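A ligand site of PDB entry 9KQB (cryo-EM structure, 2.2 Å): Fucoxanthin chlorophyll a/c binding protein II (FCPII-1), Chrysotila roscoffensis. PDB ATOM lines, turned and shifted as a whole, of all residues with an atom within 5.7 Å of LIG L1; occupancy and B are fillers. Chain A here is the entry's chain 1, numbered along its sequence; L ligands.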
ATOM      1  N   LEU A 131      19.337 -18.616 -17.810  1.00  0.00           N
ATOM      2  CA  LEU A 131      20.198 -18.921 -16.674  1.00  0.00           C
ATOM      3  C   LEU A 131      19.918 -17.986 -15.503  1.00  0.00           C
ATOM      4  O   LEU A 131      19.898 -18.424 -14.338  1.00  0.00           O
ATOM      5  CB  LEU A 131      21.667 -18.839 -17.089  1.00  0.00           C
ATOM      6  CG  LEU A 131      22.731 -18.744 -16.000  1.00  0.00           C
ATOM      7  CD1 LEU A 131      22.807 -20.041 -15.205  1.00  0.00           C
ATOM      8  CD2 LEU A 131      24.088 -18.415 -16.595  1.00  0.00           C
ATOM      9  N   ILE A 134      16.838 -18.966 -13.510  1.00  0.00           N
ATOM     10  CA  ILE A 134      17.165 -19.984 -12.525  1.00  0.00           C
ATOM     11  C   ILE A 134      17.903 -19.353 -11.343  1.00  0.00           C
ATOM     12  O   ILE A 134      17.704 -19.768 -10.194  1.00  0.00           O
ATOM     13  CB  ILE A 134      17.987 -21.097 -13.208  1.00  0.00           C
ATOM     14  CG1 ILE A 134      17.201 -21.710 -14.366  1.00  0.00           C
ATOM     15  CG2 ILE A 134      18.374 -22.188 -12.218  1.00  0.00           C
ATOM     16  CD1 ILE A 134      16.014 -22.549 -13.927  1.00  0.00           C
ATOM     17  N   ALA A 135      18.725 -18.337 -11.604  1.00  0.00           N
ATOM     18  CA  ALA A 135      19.479 -17.685 -10.542  1.00  0.00           C
ATOM     19  C   ALA A 135      18.570 -16.870  -9.626  1.00  0.00           C
ATOM     20  O   ALA A 135      18.812 -16.808  -8.415  1.00  0.00           O
ATOM     21  CB  ALA A 135      20.566 -16.791 -11.153  1.00  0.00           C
ATOM     22  N   LEU A 137      15.554 -17.494  -8.776  1.00  0.00           N
ATOM     23  CA  LEU A 137      14.850 -18.388  -7.866  1.00  0.00           C
ATOM     24  C   LEU A 137      15.690 -18.732  -6.646  1.00  0.00           C
ATOM     25  O   LEU A 137      15.190 -18.763  -5.520  1.00  0.00           O
ATOM     26  CB  LEU A 137      14.429 -19.661  -8.610  1.00  0.00           C
ATOM     27  CG  LEU A 137      12.918 -19.777  -8.823  1.00  0.00           C
ATOM     28  CD1 LEU A 137      12.463 -18.762  -9.837  1.00  0.00           C
ATOM     29  CD2 LEU A 137      12.556 -21.180  -9.269  1.00  0.00           C
ATOM     30  N   GLU A 138      16.990 -18.995  -6.855  1.00  0.00           N
ATOM     31  CA  GLU A 138      17.869 -19.300  -5.732  1.00  0.00           C
ATOM     32  C   GLU A 138      18.093 -18.073  -4.863  1.00  0.00           C
ATOM     33  O   GLU A 138      18.142 -18.168  -3.628  1.00  0.00           O
ATOM     34  CB  GLU A 138      19.195 -19.864  -6.244  1.00  0.00           C
ATOM     35  CG  GLU A 138      20.277 -19.966  -5.178  1.00  0.00           C
ATOM     36  CD  GLU A 138      19.975 -21.011  -4.125  1.00  0.00           C
ATOM     37  OE1 GLU A 138      19.225 -21.968  -4.417  1.00  0.00           O
ATOM     38  OE2 GLU A 138      20.472 -20.875  -2.983  1.00  0.00           O
ATOM     39  N   ARG A 141      14.808 -17.551  -2.932  1.00  0.00           N
ATOM     40  CA  ARG A 141      14.608 -18.626  -1.952  1.00  0.00           C
ATOM     41  C   ARG A 141      15.521 -18.449  -0.752  1.00  0.00           C
ATOM     42  O   ARG A 141      15.090 -18.609   0.400  1.00  0.00           O
ATOM     43  CB  ARG A 141      14.837 -19.984  -2.609  1.00  0.00           C
ATOM     44  CG  ARG A 141      14.953 -21.147  -1.631  1.00  0.00           C
ATOM     45  CD  ARG A 141      15.952 -22.169  -2.135  1.00  0.00           C
ATOM     46  NE  ARG A 141      17.323 -21.727  -1.938  1.00  0.00           N
ATOM     47  CZ  ARG A 141      18.107 -22.132  -0.944  1.00  0.00           C
ATOM     48  NH1 ARG A 141      17.686 -22.996  -0.035  1.00  0.00           N
ATOM     49  NH2 ARG A 141      19.339 -21.649  -0.857  1.00  0.00           N
ATOM     50  N   ASP A 153      19.185 -21.609   6.496  1.00  0.00           N
ATOM     51  CA  ASP A 153      20.012 -22.599   5.806  1.00  0.00           C
ATOM     52  C   ASP A 153      21.442 -22.622   6.321  1.00  0.00           C
ATOM     53  O   ASP A 153      22.192 -23.559   6.016  1.00  0.00           O
ATOM     54  CB  ASP A 153      19.995 -22.324   4.299  1.00  0.00           C
ATOM     55  CG  ASP A 153      20.212 -20.867   3.959  1.00  0.00           C
ATOM     56  OD1 ASP A 153      20.835 -20.130   4.755  1.00  0.00           O
ATOM     57  OD2 ASP A 153      19.757 -20.441   2.875  1.00  0.00           O
ATOM     58  N   GLY A 154      21.846 -21.613   7.094  1.00  0.00           N
ATOM     59  CA  GLY A 154      23.200 -21.526   7.598  1.00  0.00           C
ATOM     60  C   GLY A 154      24.159 -20.752   6.724  1.00  0.00           C
ATOM     61  O   GLY A 154      25.369 -20.748   7.010  1.00  0.00           O
ATOM     62  N   LEU A 155      23.676 -20.109   5.670  1.00  0.00           N
ATOM     63  CA  LEU A 155      24.528 -19.347   4.764  1.00  0.00           C
ATOM     64  C   LEU A 155      24.511 -17.843   5.054  1.00  0.00           C
ATOM     65  O   LEU A 155      25.224 -17.098   4.382  1.00  0.00           O
ATOM     66  CB  LEU A 155      24.100 -19.614   3.317  1.00  0.00           C
ATOM     67  CG  LEU A 155      24.511 -20.991   2.801  1.00  0.00           C
ATOM     68  CD1 LEU A 155      23.997 -21.242   1.395  1.00  0.00           C
ATOM     69  CD2 LEU A 155      26.027 -21.169   2.869  1.00  0.00           C
ATOM     70  N   THR A 160      25.613 -15.306  -1.156  1.00  0.00           N
ATOM     71  CA  THR A 160      26.433 -16.359  -0.567  1.00  0.00           C
ATOM     72  C   THR A 160      27.648 -16.687  -1.422  1.00  0.00           C
ATOM     73  O   THR A 160      28.758 -16.833  -0.879  1.00  0.00           O
ATOM     74  CB  THR A 160      25.565 -17.606  -0.352  1.00  0.00           C
ATOM     75  OG1 THR A 160      24.661 -17.373   0.742  1.00  0.00           O
ATOM     76  CG2 THR A 160      26.415 -18.817  -0.013  1.00  0.00           C
HETATM   77  N1  LIG L   1      20.972 -23.055  -6.419  1.00  0.00           N
HETATM   78  N2  LIG L   1      18.621 -24.906  -3.674  1.00  0.00           N
HETATM   79  C1  LIG L   1      21.598 -24.545  -2.543  1.00  0.00           C
HETATM   80  C2  LIG L   1      22.276 -22.826  -6.372  1.00  0.00           C
HETATM   81  C3  LIG L   1      18.086 -23.470  -7.366  1.00  0.00           C
HETATM   82  C4  LIG L   1      17.268 -25.369  -3.568  1.00  0.00           C
HETATM   83  C5  LIG L   1      22.961 -24.401  -1.908  1.00  0.00           C
HETATM   84  C6  LIG L   1      22.888 -22.375  -7.648  1.00  0.00           C
HETATM   85  C7  LIG L   1      16.721 -23.398  -7.944  1.00  0.00           C
HETATM   86  C8  LIG L   1      16.918 -26.072  -2.302  1.00  0.00           C
HETATM   87  C9  LIG L   1      23.744 -23.683  -2.990  1.00  0.00           C
HETATM   88  C10 LIG L   1      21.713 -22.336  -8.540  1.00  0.00           C
HETATM   89  C11 LIG L   1      15.887 -24.044  -6.932  1.00  0.00           C
HETATM   90  C12 LIG L   1      18.238 -25.994  -1.604  1.00  0.00           C
HETATM   91  C13 LIG L   1      22.689 -23.604  -4.035  1.00  0.00           C
HETATM   92  C14 LIG L   1      20.584 -22.775  -7.669  1.00  0.00           C
HETATM   93  C15 LIG L   1      16.872 -24.420  -5.884  1.00  0.00           C
HETATM   94  C16 LIG L   1      19.123 -25.351  -2.459  1.00  0.00           C
HETATM   95  C17 LIG L   1      23.679 -25.749  -1.756  1.00  0.00           C
HETATM   96  C18 LIG L   1      21.668 -21.947  -9.964  1.00  0.00           C
HETATM   97  C19 LIG L   1      14.393 -24.276  -6.957  1.00  0.00           C
HETATM   98  C20 LIG L   1      18.981 -26.360  -0.373  1.00  0.00           C
HETATM   99  C21 LIG L   1      25.129 -25.608  -1.311  1.00  0.00           C
HETATM  100  C22 LIG L   1      21.041 -20.852 -10.325  1.00  0.00           C
HETATM  101  C23 LIG L   1      14.177 -25.539  -7.747  1.00  0.00           C
HETATM  102  C24 LIG L   1      20.381 -25.881  -0.490  1.00  0.00           C
HETATM  103  C25 LIG L   1      22.298 -24.540   2.480  1.00  0.00           C
HETATM  104  C26 LIG L   1      25.225 -25.676   0.191  1.00  0.00           C
HETATM  105  C27 LIG L   1      20.680 -24.925   0.623  1.00  0.00           C
HETATM  106  C28 LIG L   1      20.455 -25.212  -1.827  1.00  0.00           C
HETATM  107  C29 LIG L   1      23.079 -23.034  -5.165  1.00  0.00           C
HETATM  108  C30 LIG L   1      19.198 -22.891  -8.141  1.00  0.00           C
HETATM  109  C31 LIG L   1      16.344 -25.110  -4.684  1.00  0.00           C
HETATM  110  C32 LIG L   1      24.073 -22.263  -2.542  1.00  0.00           C
HETATM  111  C33 LIG L   1      24.319 -22.030  -7.948  1.00  0.00           C
HETATM  112  C34 LIG L   1      16.286 -22.797  -9.256  1.00  0.00           C
HETATM  113  C35 LIG L   1      15.698 -26.722  -1.712  1.00  0.00           C
HETATM  114  N3  LIG L   1      21.488 -24.114  -3.747  1.00  0.00           N
HETATM  115  N4  LIG L   1      18.152 -24.062  -6.162  1.00  0.00           N
HETATM  116  O1  LIG L   1      24.914 -26.688   0.781  1.00  0.00           O
HETATM  117  O2  LIG L   1      20.364 -23.752   0.546  1.00  0.00           O
HETATM  118  O3  LIG L   1      25.714 -24.534   0.952  1.00  0.00           O
HETATM  119  O4  LIG L   1      21.402 -25.400   1.787  1.00  0.00           O
HETATM  120  O5  LIG L   1      18.493 -26.987   0.640  1.00  0.00           O
HETATM  121 MG1  LIG L   1      19.803 -23.833  -4.929  1.00  0.00          MG
HETATM  122 MG1  LG2 L   2      31.732 -18.203  -5.498  1.00  0.00          MG
HETATM  123  C1  LG2 L   2      29.581 -20.781  -4.173  1.00  0.00           C
HETATM  124  C2  LG2 L   2      33.692 -18.794  -2.658  1.00  0.00           C
HETATM  125  C3  LG2 L   2      34.090 -16.087  -6.862  1.00  0.00           C
HETATM  126  C4  LG2 L   2      29.700 -17.843  -8.308  1.00  0.00           C
HETATM  127  N1  LG2 L   2      31.692 -19.624  -3.652  1.00  0.00           N
HETATM  128  C5  LG2 L   2      30.805 -20.490  -3.371  1.00  0.00           C
HETATM  129  C6  LG2 L   2      31.084 -21.224  -2.098  1.00  0.00           C
HETATM  130  C7  LG2 L   2      32.233 -20.432  -1.515  1.00  0.00           C
HETATM  131  C8  LG2 L   2      32.586 -19.552  -2.665  1.00  0.00           C
HETATM  132  C9  LG2 L   2      31.782 -19.591  -0.327  1.00  0.00           C
HETATM  133  C10 LG2 L   2      31.506 -22.655  -2.367  1.00  0.00           C
HETATM  134  N2  LG2 L   2      33.540 -17.599  -4.839  1.00  0.00           N
HETATM  135  C11 LG2 L   2      34.214 -17.881  -3.708  1.00  0.00           C
HETATM  136  C12 LG2 L   2      35.524 -17.194  -3.585  1.00  0.00           C
HETATM  137  C13 LG2 L   2      35.582 -16.419  -4.839  1.00  0.00           C
HETATM  138  C14 LG2 L   2      34.307 -16.739  -5.544  1.00  0.00           C
HETATM  139  C15 LG2 L   2      36.529 -17.267  -2.471  1.00  0.00           C
HETATM  140  C16 LG2 L   2      36.563 -15.489  -5.450  1.00  0.00           C
HETATM  141  C17 LG2 L   2      37.118 -14.538  -4.721  1.00  0.00           C
HETATM  142  N3  LG2 L   2      31.927 -17.125  -7.317  1.00  0.00           N
HETATM  143  C18 LG2 L   2      32.877 -16.269  -7.700  1.00  0.00           C
HETATM  144  C19 LG2 L   2      32.601 -15.566  -8.977  1.00  0.00           C
HETATM  145  C20 LG2 L   2      31.291 -16.127  -9.355  1.00  0.00           C
HETATM  146  C21 LG2 L   2      30.968 -17.084  -8.256  1.00  0.00           C
HETATM  147  C22 LG2 L   2      33.439 -14.544  -9.698  1.00  0.00           C
HETATM  148  C23 LG2 L   2      30.461 -15.794 -10.585  1.00  0.00           C
HETATM  149  C24 LG2 L   2      30.610 -16.886 -11.618  1.00  0.00           C
HETATM  150  N4  LG2 L   2      30.086 -19.037  -6.187  1.00  0.00           N
HETATM  151  C25 LG2 L   2      29.327 -18.819  -7.269  1.00  0.00           C
HETATM  152  C26 LG2 L   2      28.103 -19.649  -7.293  1.00  0.00           C
HETATM  153  C27 LG2 L   2      28.229 -20.429  -6.037  1.00  0.00           C
HETATM  154  C28 LG2 L   2      29.423 -20.018  -5.441  1.00  0.00           C
HETATM  155  C29 LG2 L   2      27.035 -19.656  -8.348  1.00  0.00           C
HETATM  156  C30 LG2 L   2      27.572 -21.471  -5.185  1.00  0.00           C
HETATM  157  O1  LG2 L   2      26.468 -22.078  -5.422  1.00  0.00           O
HETATM  158  C31 LG2 L   2      28.349 -21.562  -3.937  1.00  0.00           C
HETATM  159  C32 LG2 L   2      27.547 -20.943  -2.840  1.00  0.00           C
HETATM  160  O2  LG2 L   2      26.915 -19.935  -3.056  1.00  0.00           O
HETATM  161  O3  LG2 L   2      27.400 -21.602  -1.554  1.00  0.00           O
HETATM  162  C33 LG2 L   2      27.829 -22.954  -1.364  1.00  0.00           C
HETATM  163 MG1  LG3 L   3      11.168 -22.599   0.363  1.00  0.00          MG
HETATM  164  C1  LG3 L   3       9.809 -22.058   3.786  1.00  0.00           C
HETATM  165  C2  LG3 L   3      11.821 -25.473   1.082  1.00  0.00           C
HETATM  166  C3  LG3 L   3      11.908 -22.520  -2.947  1.00  0.00           C
HETATM  167  C4  LG3 L   3       9.873 -18.938  -0.213  1.00  0.00           C
HETATM  168  N1  LG3 L   3      10.764 -23.647   2.179  1.00  0.00           N
HETATM  169  C5  LG3 L   3      10.266 -23.398   3.316  1.00  0.00           C
HETATM  170  C6  LG3 L   3      10.207 -24.604   4.207  1.00  0.00           C
HETATM  171  C7  LG3 L   3      10.945 -25.639   3.397  1.00  0.00           C
HETATM  172  C8  LG3 L   3      11.208 -24.898   2.127  1.00  0.00           C
HETATM  173  C9  LG3 L   3      12.267 -26.032   4.051  1.00  0.00           C
HETATM  174  C10 LG3 L   3       8.774 -25.044   4.497  1.00  0.00           C
HETATM  175  C11 LG3 L   3       7.907 -24.977   3.247  1.00  0.00           C
HETATM  176  C12 LG3 L   3       6.508 -25.466   3.522  1.00  0.00           C
HETATM  177  O1  LG3 L   3       5.821 -24.976   4.399  1.00  0.00           O
HETATM  178  O2  LG3 L   3       5.981 -26.553   2.703  1.00  0.00           O
HETATM  179  N2  LG3 L   3      11.873 -23.736  -0.679  1.00  0.00           N
HETATM  180  C13 LG3 L   3      11.794 -25.038  -0.333  1.00  0.00           C
HETATM  181  C14 LG3 L   3      11.738 -25.968  -1.491  1.00  0.00           C
HETATM  182  C15 LG3 L   3      11.768 -25.032  -2.641  1.00  0.00           C
HETATM  183  C16 LG3 L   3      11.857 -23.679  -2.036  1.00  0.00           C
HETATM  184  C17 LG3 L   3      11.639 -27.458  -1.465  1.00  0.00           C
HETATM  185  C18 LG3 L   3      11.724 -25.197  -4.111  1.00  0.00           C
HETATM  186  C19 LG3 L   3      12.334 -26.200  -4.710  1.00  0.00           C
HETATM  187  N3  LG3 L   3      10.928 -20.939  -1.364  1.00  0.00           N
HETATM  188  C20 LG3 L   3      11.315 -21.205  -2.614  1.00  0.00           C
HETATM  189  C21 LG3 L   3      11.086 -20.095  -3.572  1.00  0.00           C
HETATM  190  C22 LG3 L   3      10.479 -19.051  -2.713  1.00  0.00           C
HETATM  191  C23 LG3 L   3      10.425 -19.684  -1.355  1.00  0.00           C
HETATM  192  C24 LG3 L   3      11.397 -20.044  -5.044  1.00  0.00           C
HETATM  193  C25 LG3 L   3      10.024 -17.677  -3.141  1.00  0.00           C
HETATM  194  C26 LG3 L   3      10.926 -16.592  -2.612  1.00  0.00           C
HETATM  195  N4  LG3 L   3      10.008 -20.792   1.387  1.00  0.00           N
HETATM  196  C27 LG3 L   3       9.720 -19.501   1.146  1.00  0.00           C
HETATM  197  C28 LG3 L   3       9.260 -18.764   2.338  1.00  0.00           C
HETATM  198  C29 LG3 L   3       9.305 -19.811   3.385  1.00  0.00           C
HETATM  199  C30 LG3 L   3       9.744 -20.979   2.756  1.00  0.00           C
HETATM  200  C31 LG3 L   3       8.857 -17.320   2.445  1.00  0.00           C
HETATM  201  C32 LG3 L   3       9.054 -20.074   4.830  1.00  0.00           C
HETATM  202  O3  LG3 L   3       8.636 -19.237   5.703  1.00  0.00           O
HETATM  203  C33 LG3 L   3       9.441 -21.478   5.100  1.00  0.00           C
HETATM  204  C34 LG3 L   3      10.620 -21.490   6.027  1.00  0.00           C
HETATM  205  O4  LG3 L   3      11.605 -20.808   5.780  1.00  0.00           O
HETATM  206  O5  LG3 L   3      10.628 -22.343   7.205  1.00  0.00           O
HETATM  207  C35 LG3 L   3       9.460 -23.041   7.610  1.00  0.00           C
HETATM  208  C36 LG3 L   3       4.666 -26.450   2.141  1.00  0.00           C
HETATM  209  C37 LG3 L   3       4.822 -25.756   0.816  1.00  0.00           C
HETATM  210  C38 LG3 L   3       4.152 -26.105  -0.283  1.00  0.00           C
HETATM  211  C39 LG3 L   3       4.393 -25.335  -1.546  1.00  0.00           C
HETATM  212  C40 LG3 L   3       3.169 -27.259  -0.246  1.00  0.00           C
HETATM  213  C41 LG3 L   3       2.839 -27.780  -1.644  1.00  0.00           C
HETATM  214  C42 LG3 L   3       1.426 -27.401  -2.083  1.00  0.00           C
HETATM  215  C43 LG3 L   3       1.269 -27.538  -3.592  1.00  0.00           C
HETATM  216  C44 LG3 L   3       2.260 -26.641  -4.332  1.00  0.00           C
HETATM  217  C45 LG3 L   3      -0.162 -27.204  -3.988  1.00  0.00           C
HETATM  218  C1  LG4 L   4      17.230 -28.912  -5.492  1.00  0.00           C
HETATM  219  O1  LG4 L   4      21.062 -23.750 -15.475  1.00  0.00           O
HETATM  220  C2  LG4 L   4      15.846 -29.014  -5.999  1.00  0.00           C
HETATM  221  C3  LG4 L   4      20.378 -25.308 -13.378  1.00  0.00           C
HETATM  222  C4  LG4 L   4      19.744 -25.321 -14.577  1.00  0.00           C
HETATM  223  C5  LG4 L   4      18.590 -26.223 -14.814  1.00  0.00           C
HETATM  224  C6  LG4 L   4      20.093 -24.504 -15.619  1.00  0.00           C
HETATM  225  C7  LG4 L   4      19.311 -24.443 -16.912  1.00  0.00           C
HETATM  226  C8  LG4 L   4      20.104 -24.612 -18.177  1.00  0.00           C
HETATM  227  C9  LG4 L   4      20.223 -23.329 -19.033  1.00  0.00           C
HETATM  228  C10 LG4 L   4      19.994 -23.676 -20.506  1.00  0.00           C
HETATM  229  C11 LG4 L   4      20.873 -24.805 -20.998  1.00  0.00           C
HETATM  230  C12 LG4 L   4      20.559 -26.098 -20.263  1.00  0.00           C
HETATM  231  C13 LG4 L   4      15.636 -28.919  -7.383  1.00  0.00           C
HETATM  232  C14 LG4 L   4      20.247 -25.954 -18.792  1.00  0.00           C
HETATM  233  C15 LG4 L   4      19.659 -27.173 -18.163  1.00  0.00           C
HETATM  234  C16 LG4 L   4      19.172 -22.295 -18.637  1.00  0.00           C
HETATM  235  C17 LG4 L   4      21.604 -22.679 -18.935  1.00  0.00           C
HETATM  236  C18 LG4 L   4      14.816 -29.198  -5.053  1.00  0.00           C
HETATM  237  C19 LG4 L   4      14.910 -29.730  -3.773  1.00  0.00           C
HETATM  238  C20 LG4 L   4      14.251 -30.799  -3.216  1.00  0.00           C
HETATM  239  C21 LG4 L   4      12.881 -31.102  -3.225  1.00  0.00           C
HETATM  240  C22 LG4 L   4      12.323 -31.837  -4.384  1.00  0.00           C
HETATM  241  C23 LG4 L   4      11.933 -30.730  -2.175  1.00  0.00           C
HETATM  242  C24 LG4 L   4      16.589 -28.788  -8.387  1.00  0.00           C
HETATM  243  C25 LG4 L   4      11.879 -31.351  -1.028  1.00  0.00           C
HETATM  244  C26 LG4 L   4      11.876 -32.021   0.092  1.00  0.00           C
HETATM  245  C27 LG4 L   4      11.180 -33.380   0.178  1.00  0.00           C
HETATM  246  C28 LG4 L   4      11.182 -33.883   1.633  1.00  0.00           C
HETATM  247  C29 LG4 L   4      10.863 -32.859   2.708  1.00  0.00           C
HETATM  248  C30 LG4 L   4      11.562 -31.518   2.522  1.00  0.00           C
HETATM  249  C31 LG4 L   4      12.542 -31.447   1.350  1.00  0.00           C
HETATM  250  C32 LG4 L   4      13.015 -30.016   1.160  1.00  0.00           C
HETATM  251  C33 LG4 L   4       8.581 -33.529   3.136  1.00  0.00           C
HETATM  252  C34 LG4 L   4       7.246 -33.385   2.486  1.00  0.00           C
HETATM  253  C35 LG4 L   4      16.794 -27.787  -9.331  1.00  0.00           C
HETATM  254  C36 LG4 L   4       9.741 -33.277  -0.342  1.00  0.00           C
HETATM  255  C37 LG4 L   4      11.913 -34.400  -0.707  1.00  0.00           C
HETATM  256  C38 LG4 L   4      17.895 -27.002  -9.609  1.00  0.00           C
HETATM  257  C39 LG4 L   4      18.105 -26.156 -10.718  1.00  0.00           C
HETATM  258  C40 LG4 L   4      16.911 -25.760 -11.507  1.00  0.00           C
HETATM  259  C41 LG4 L   4      19.369 -25.692 -11.130  1.00  0.00           C
HETATM  260  C42 LG4 L   4      20.100 -26.056 -12.239  1.00  0.00           C
HETATM  261  O2  LG4 L   4      21.339 -25.362 -18.033  1.00  0.00           O
HETATM  262  O3  LG4 L   4      20.672 -24.999 -22.394  1.00  0.00           O
HETATM  263  O4  LG4 L   4      13.674 -32.258   1.732  1.00  0.00           O
HETATM  264  O5  LG4 L   4       9.433 -32.569   2.726  1.00  0.00           O
HETATM  265  O6  LG4 L   4       8.874 -34.373   3.933  1.00  0.00           O
HETATM  266  C1  LG5 L   5      23.072  -7.153 -17.333  1.00  0.00           C
HETATM  267  O1  LG5 L   5      23.415 -15.178 -10.364  1.00  0.00           O
HETATM  268  C2  LG5 L   5      23.358  -8.219 -18.331  1.00  0.00           C
HETATM  269  C3  LG5 L   5      23.544 -15.873 -12.961  1.00  0.00           C
HETATM  270  C4  LG5 L   5      24.078 -16.590 -11.952  1.00  0.00           C
HETATM  271  C5  LG5 L   5      24.797 -17.856 -12.232  1.00  0.00           C
HETATM  272  C6  LG5 L   5      23.991 -16.225 -10.627  1.00  0.00           C
HETATM  273  C7  LG5 L   5      24.551 -17.046  -9.486  1.00  0.00           C
HETATM  274  C8  LG5 L   5      24.395 -16.482  -8.089  1.00  0.00           C
HETATM  275  C9  LG5 L   5      25.513 -15.523  -7.631  1.00  0.00           C
HETATM  276  C10 LG5 L   5      25.837 -15.758  -6.152  1.00  0.00           C
HETATM  277  C11 LG5 L   5      24.613 -15.870  -5.273  1.00  0.00           C
HETATM  278  C12 LG5 L   5      23.805 -17.098  -5.652  1.00  0.00           C
HETATM  279  C13 LG5 L   5      23.307  -9.564 -17.909  1.00  0.00           C
HETATM  280  C14 LG5 L   5      23.551 -17.222  -7.128  1.00  0.00           C
HETATM  281  C15 LG5 L   5      22.779 -18.451  -7.533  1.00  0.00           C
HETATM  282  C16 LG5 L   5      26.812 -15.672  -8.424  1.00  0.00           C
HETATM  283  C17 LG5 L   5      25.039 -14.068  -7.732  1.00  0.00           C
HETATM  284  C18 LG5 L   5      23.649  -7.824 -19.656  1.00  0.00           C
HETATM  285  C19 LG5 L   5      23.296  -6.664 -20.314  1.00  0.00           C
HETATM  286  C20 LG5 L   5      23.171  -6.471 -21.682  1.00  0.00           C
HETATM  287  C21 LG5 L   5      22.802  -5.333 -22.385  1.00  0.00           C
HETATM  288  C22 LG5 L   5      22.533  -4.085 -21.626  1.00  0.00           C
HETATM  289  C23 LG5 L   5      22.625  -5.266 -23.831  1.00  0.00           C
HETATM  290  C24 LG5 L   5      23.078 -10.053 -16.636  1.00  0.00           C
HETATM  291  C25 LG5 L   5      22.769  -4.192 -24.563  1.00  0.00           C
HETATM  292  C26 LG5 L   5      22.950  -3.060 -25.179  1.00  0.00           C
HETATM  293  C27 LG5 L   5      21.754  -2.145 -25.459  1.00  0.00           C
HETATM  294  C28 LG5 L   5      22.251  -0.823 -26.075  1.00  0.00           C
HETATM  295  C29 LG5 L   5      23.471  -0.286 -25.376  1.00  0.00           C
HETATM  296  C30 LG5 L   5      24.658  -1.213 -25.527  1.00  0.00           C
HETATM  297  C31 LG5 L   5      24.363  -2.692 -25.668  1.00  0.00           C
HETATM  298  C32 LG5 L   5      24.640  -3.170 -27.082  1.00  0.00           C
HETATM  299  C33 LG5 L   5      23.287   2.120 -25.616  1.00  0.00           C
HETATM  300  C34 LG5 L   5      23.419   2.329 -24.139  1.00  0.00           C
HETATM  301  C35 LG5 L   5      23.487 -11.232 -16.014  1.00  0.00           C
HETATM  302  C36 LG5 L   5      20.774  -2.824 -26.436  1.00  0.00           C
HETATM  303  C37 LG5 L   5      21.013  -1.839 -24.159  1.00  0.00           C
HETATM  304  C38 LG5 L   5      22.874 -12.463 -15.855  1.00  0.00           C
HETATM  305  C39 LG5 L   5      23.460 -13.726 -15.700  1.00  0.00           C
HETATM  306  C40 LG5 L   5      23.266 -14.730 -16.767  1.00  0.00           C
HETATM  307  C41 LG5 L   5      24.242 -14.099 -14.588  1.00  0.00           C
HETATM  308  C42 LG5 L   5      23.819 -14.573 -13.359  1.00  0.00           C
HETATM  309  O2  LG5 L   5      23.055 -16.005  -7.754  1.00  0.00           O
HETATM  310  O3  LG5 L   5      25.014 -15.960  -3.900  1.00  0.00           O
HETATM  311  O4  LG5 L   5      25.315  -3.331 -24.785  1.00  0.00           O
HETATM  312  O5  LG5 L   5      23.871   0.968 -26.003  1.00  0.00           O
HETATM  313  O6  LG5 L   5      22.755   2.874 -26.375  1.00  0.00           O
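A magnesium atom (MG1) of LIG L1 is bound by the side-chain carboxylate (OE1) of Glu 138 (2.0 Å).
The guanidinium group (NH2) of Arg 141 is in hydrogen-bond range of an oxygen (O2) of LIG L1 (2.7 Å).
An oxygen (O3) of LG5 L5 sits at hydrogen-bond distance from the backbone NH of Thr 160, 2.9 Å away.
OE2 of Glu 138 is in salt-bridge range of NH2 of Arg 141 (2.5 Å).
NH2 of Arg 141 is in salt-bridge range of OD2 of Asp 153 (3.9 Å).
N of Leu 155 lies within hydrogen-bond range of OD1 of Asp 153 (3.0 Å).
O of Ile 134 touches C34 of LIG L1, 3.5 Å away.
CA of Ala 135 touches C22 of LIG L1, at 3.5 Å.
CB of Leu 137 touches C34 of LIG L1 (3.7 Å).
Asp 153 touches LIG L1 (O to C25, 3.7 Å).
CD1 of Leu 155 touches O3 of LIG L1, at 3.7 Å.
Hydrophobic or aromatic side chains within 4 Å of LIG L1: Ile 134, Leu 137 and Leu 155.
Seven residues have an atom within 4 Å of LIG L1: Ile 134, Ala 135, Leu 137, Glu 138, Arg 141, Asp 153 and Leu 155.
The nearest printed residue that does not touch LIG L1 is Leu 131 (4.8 Å).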
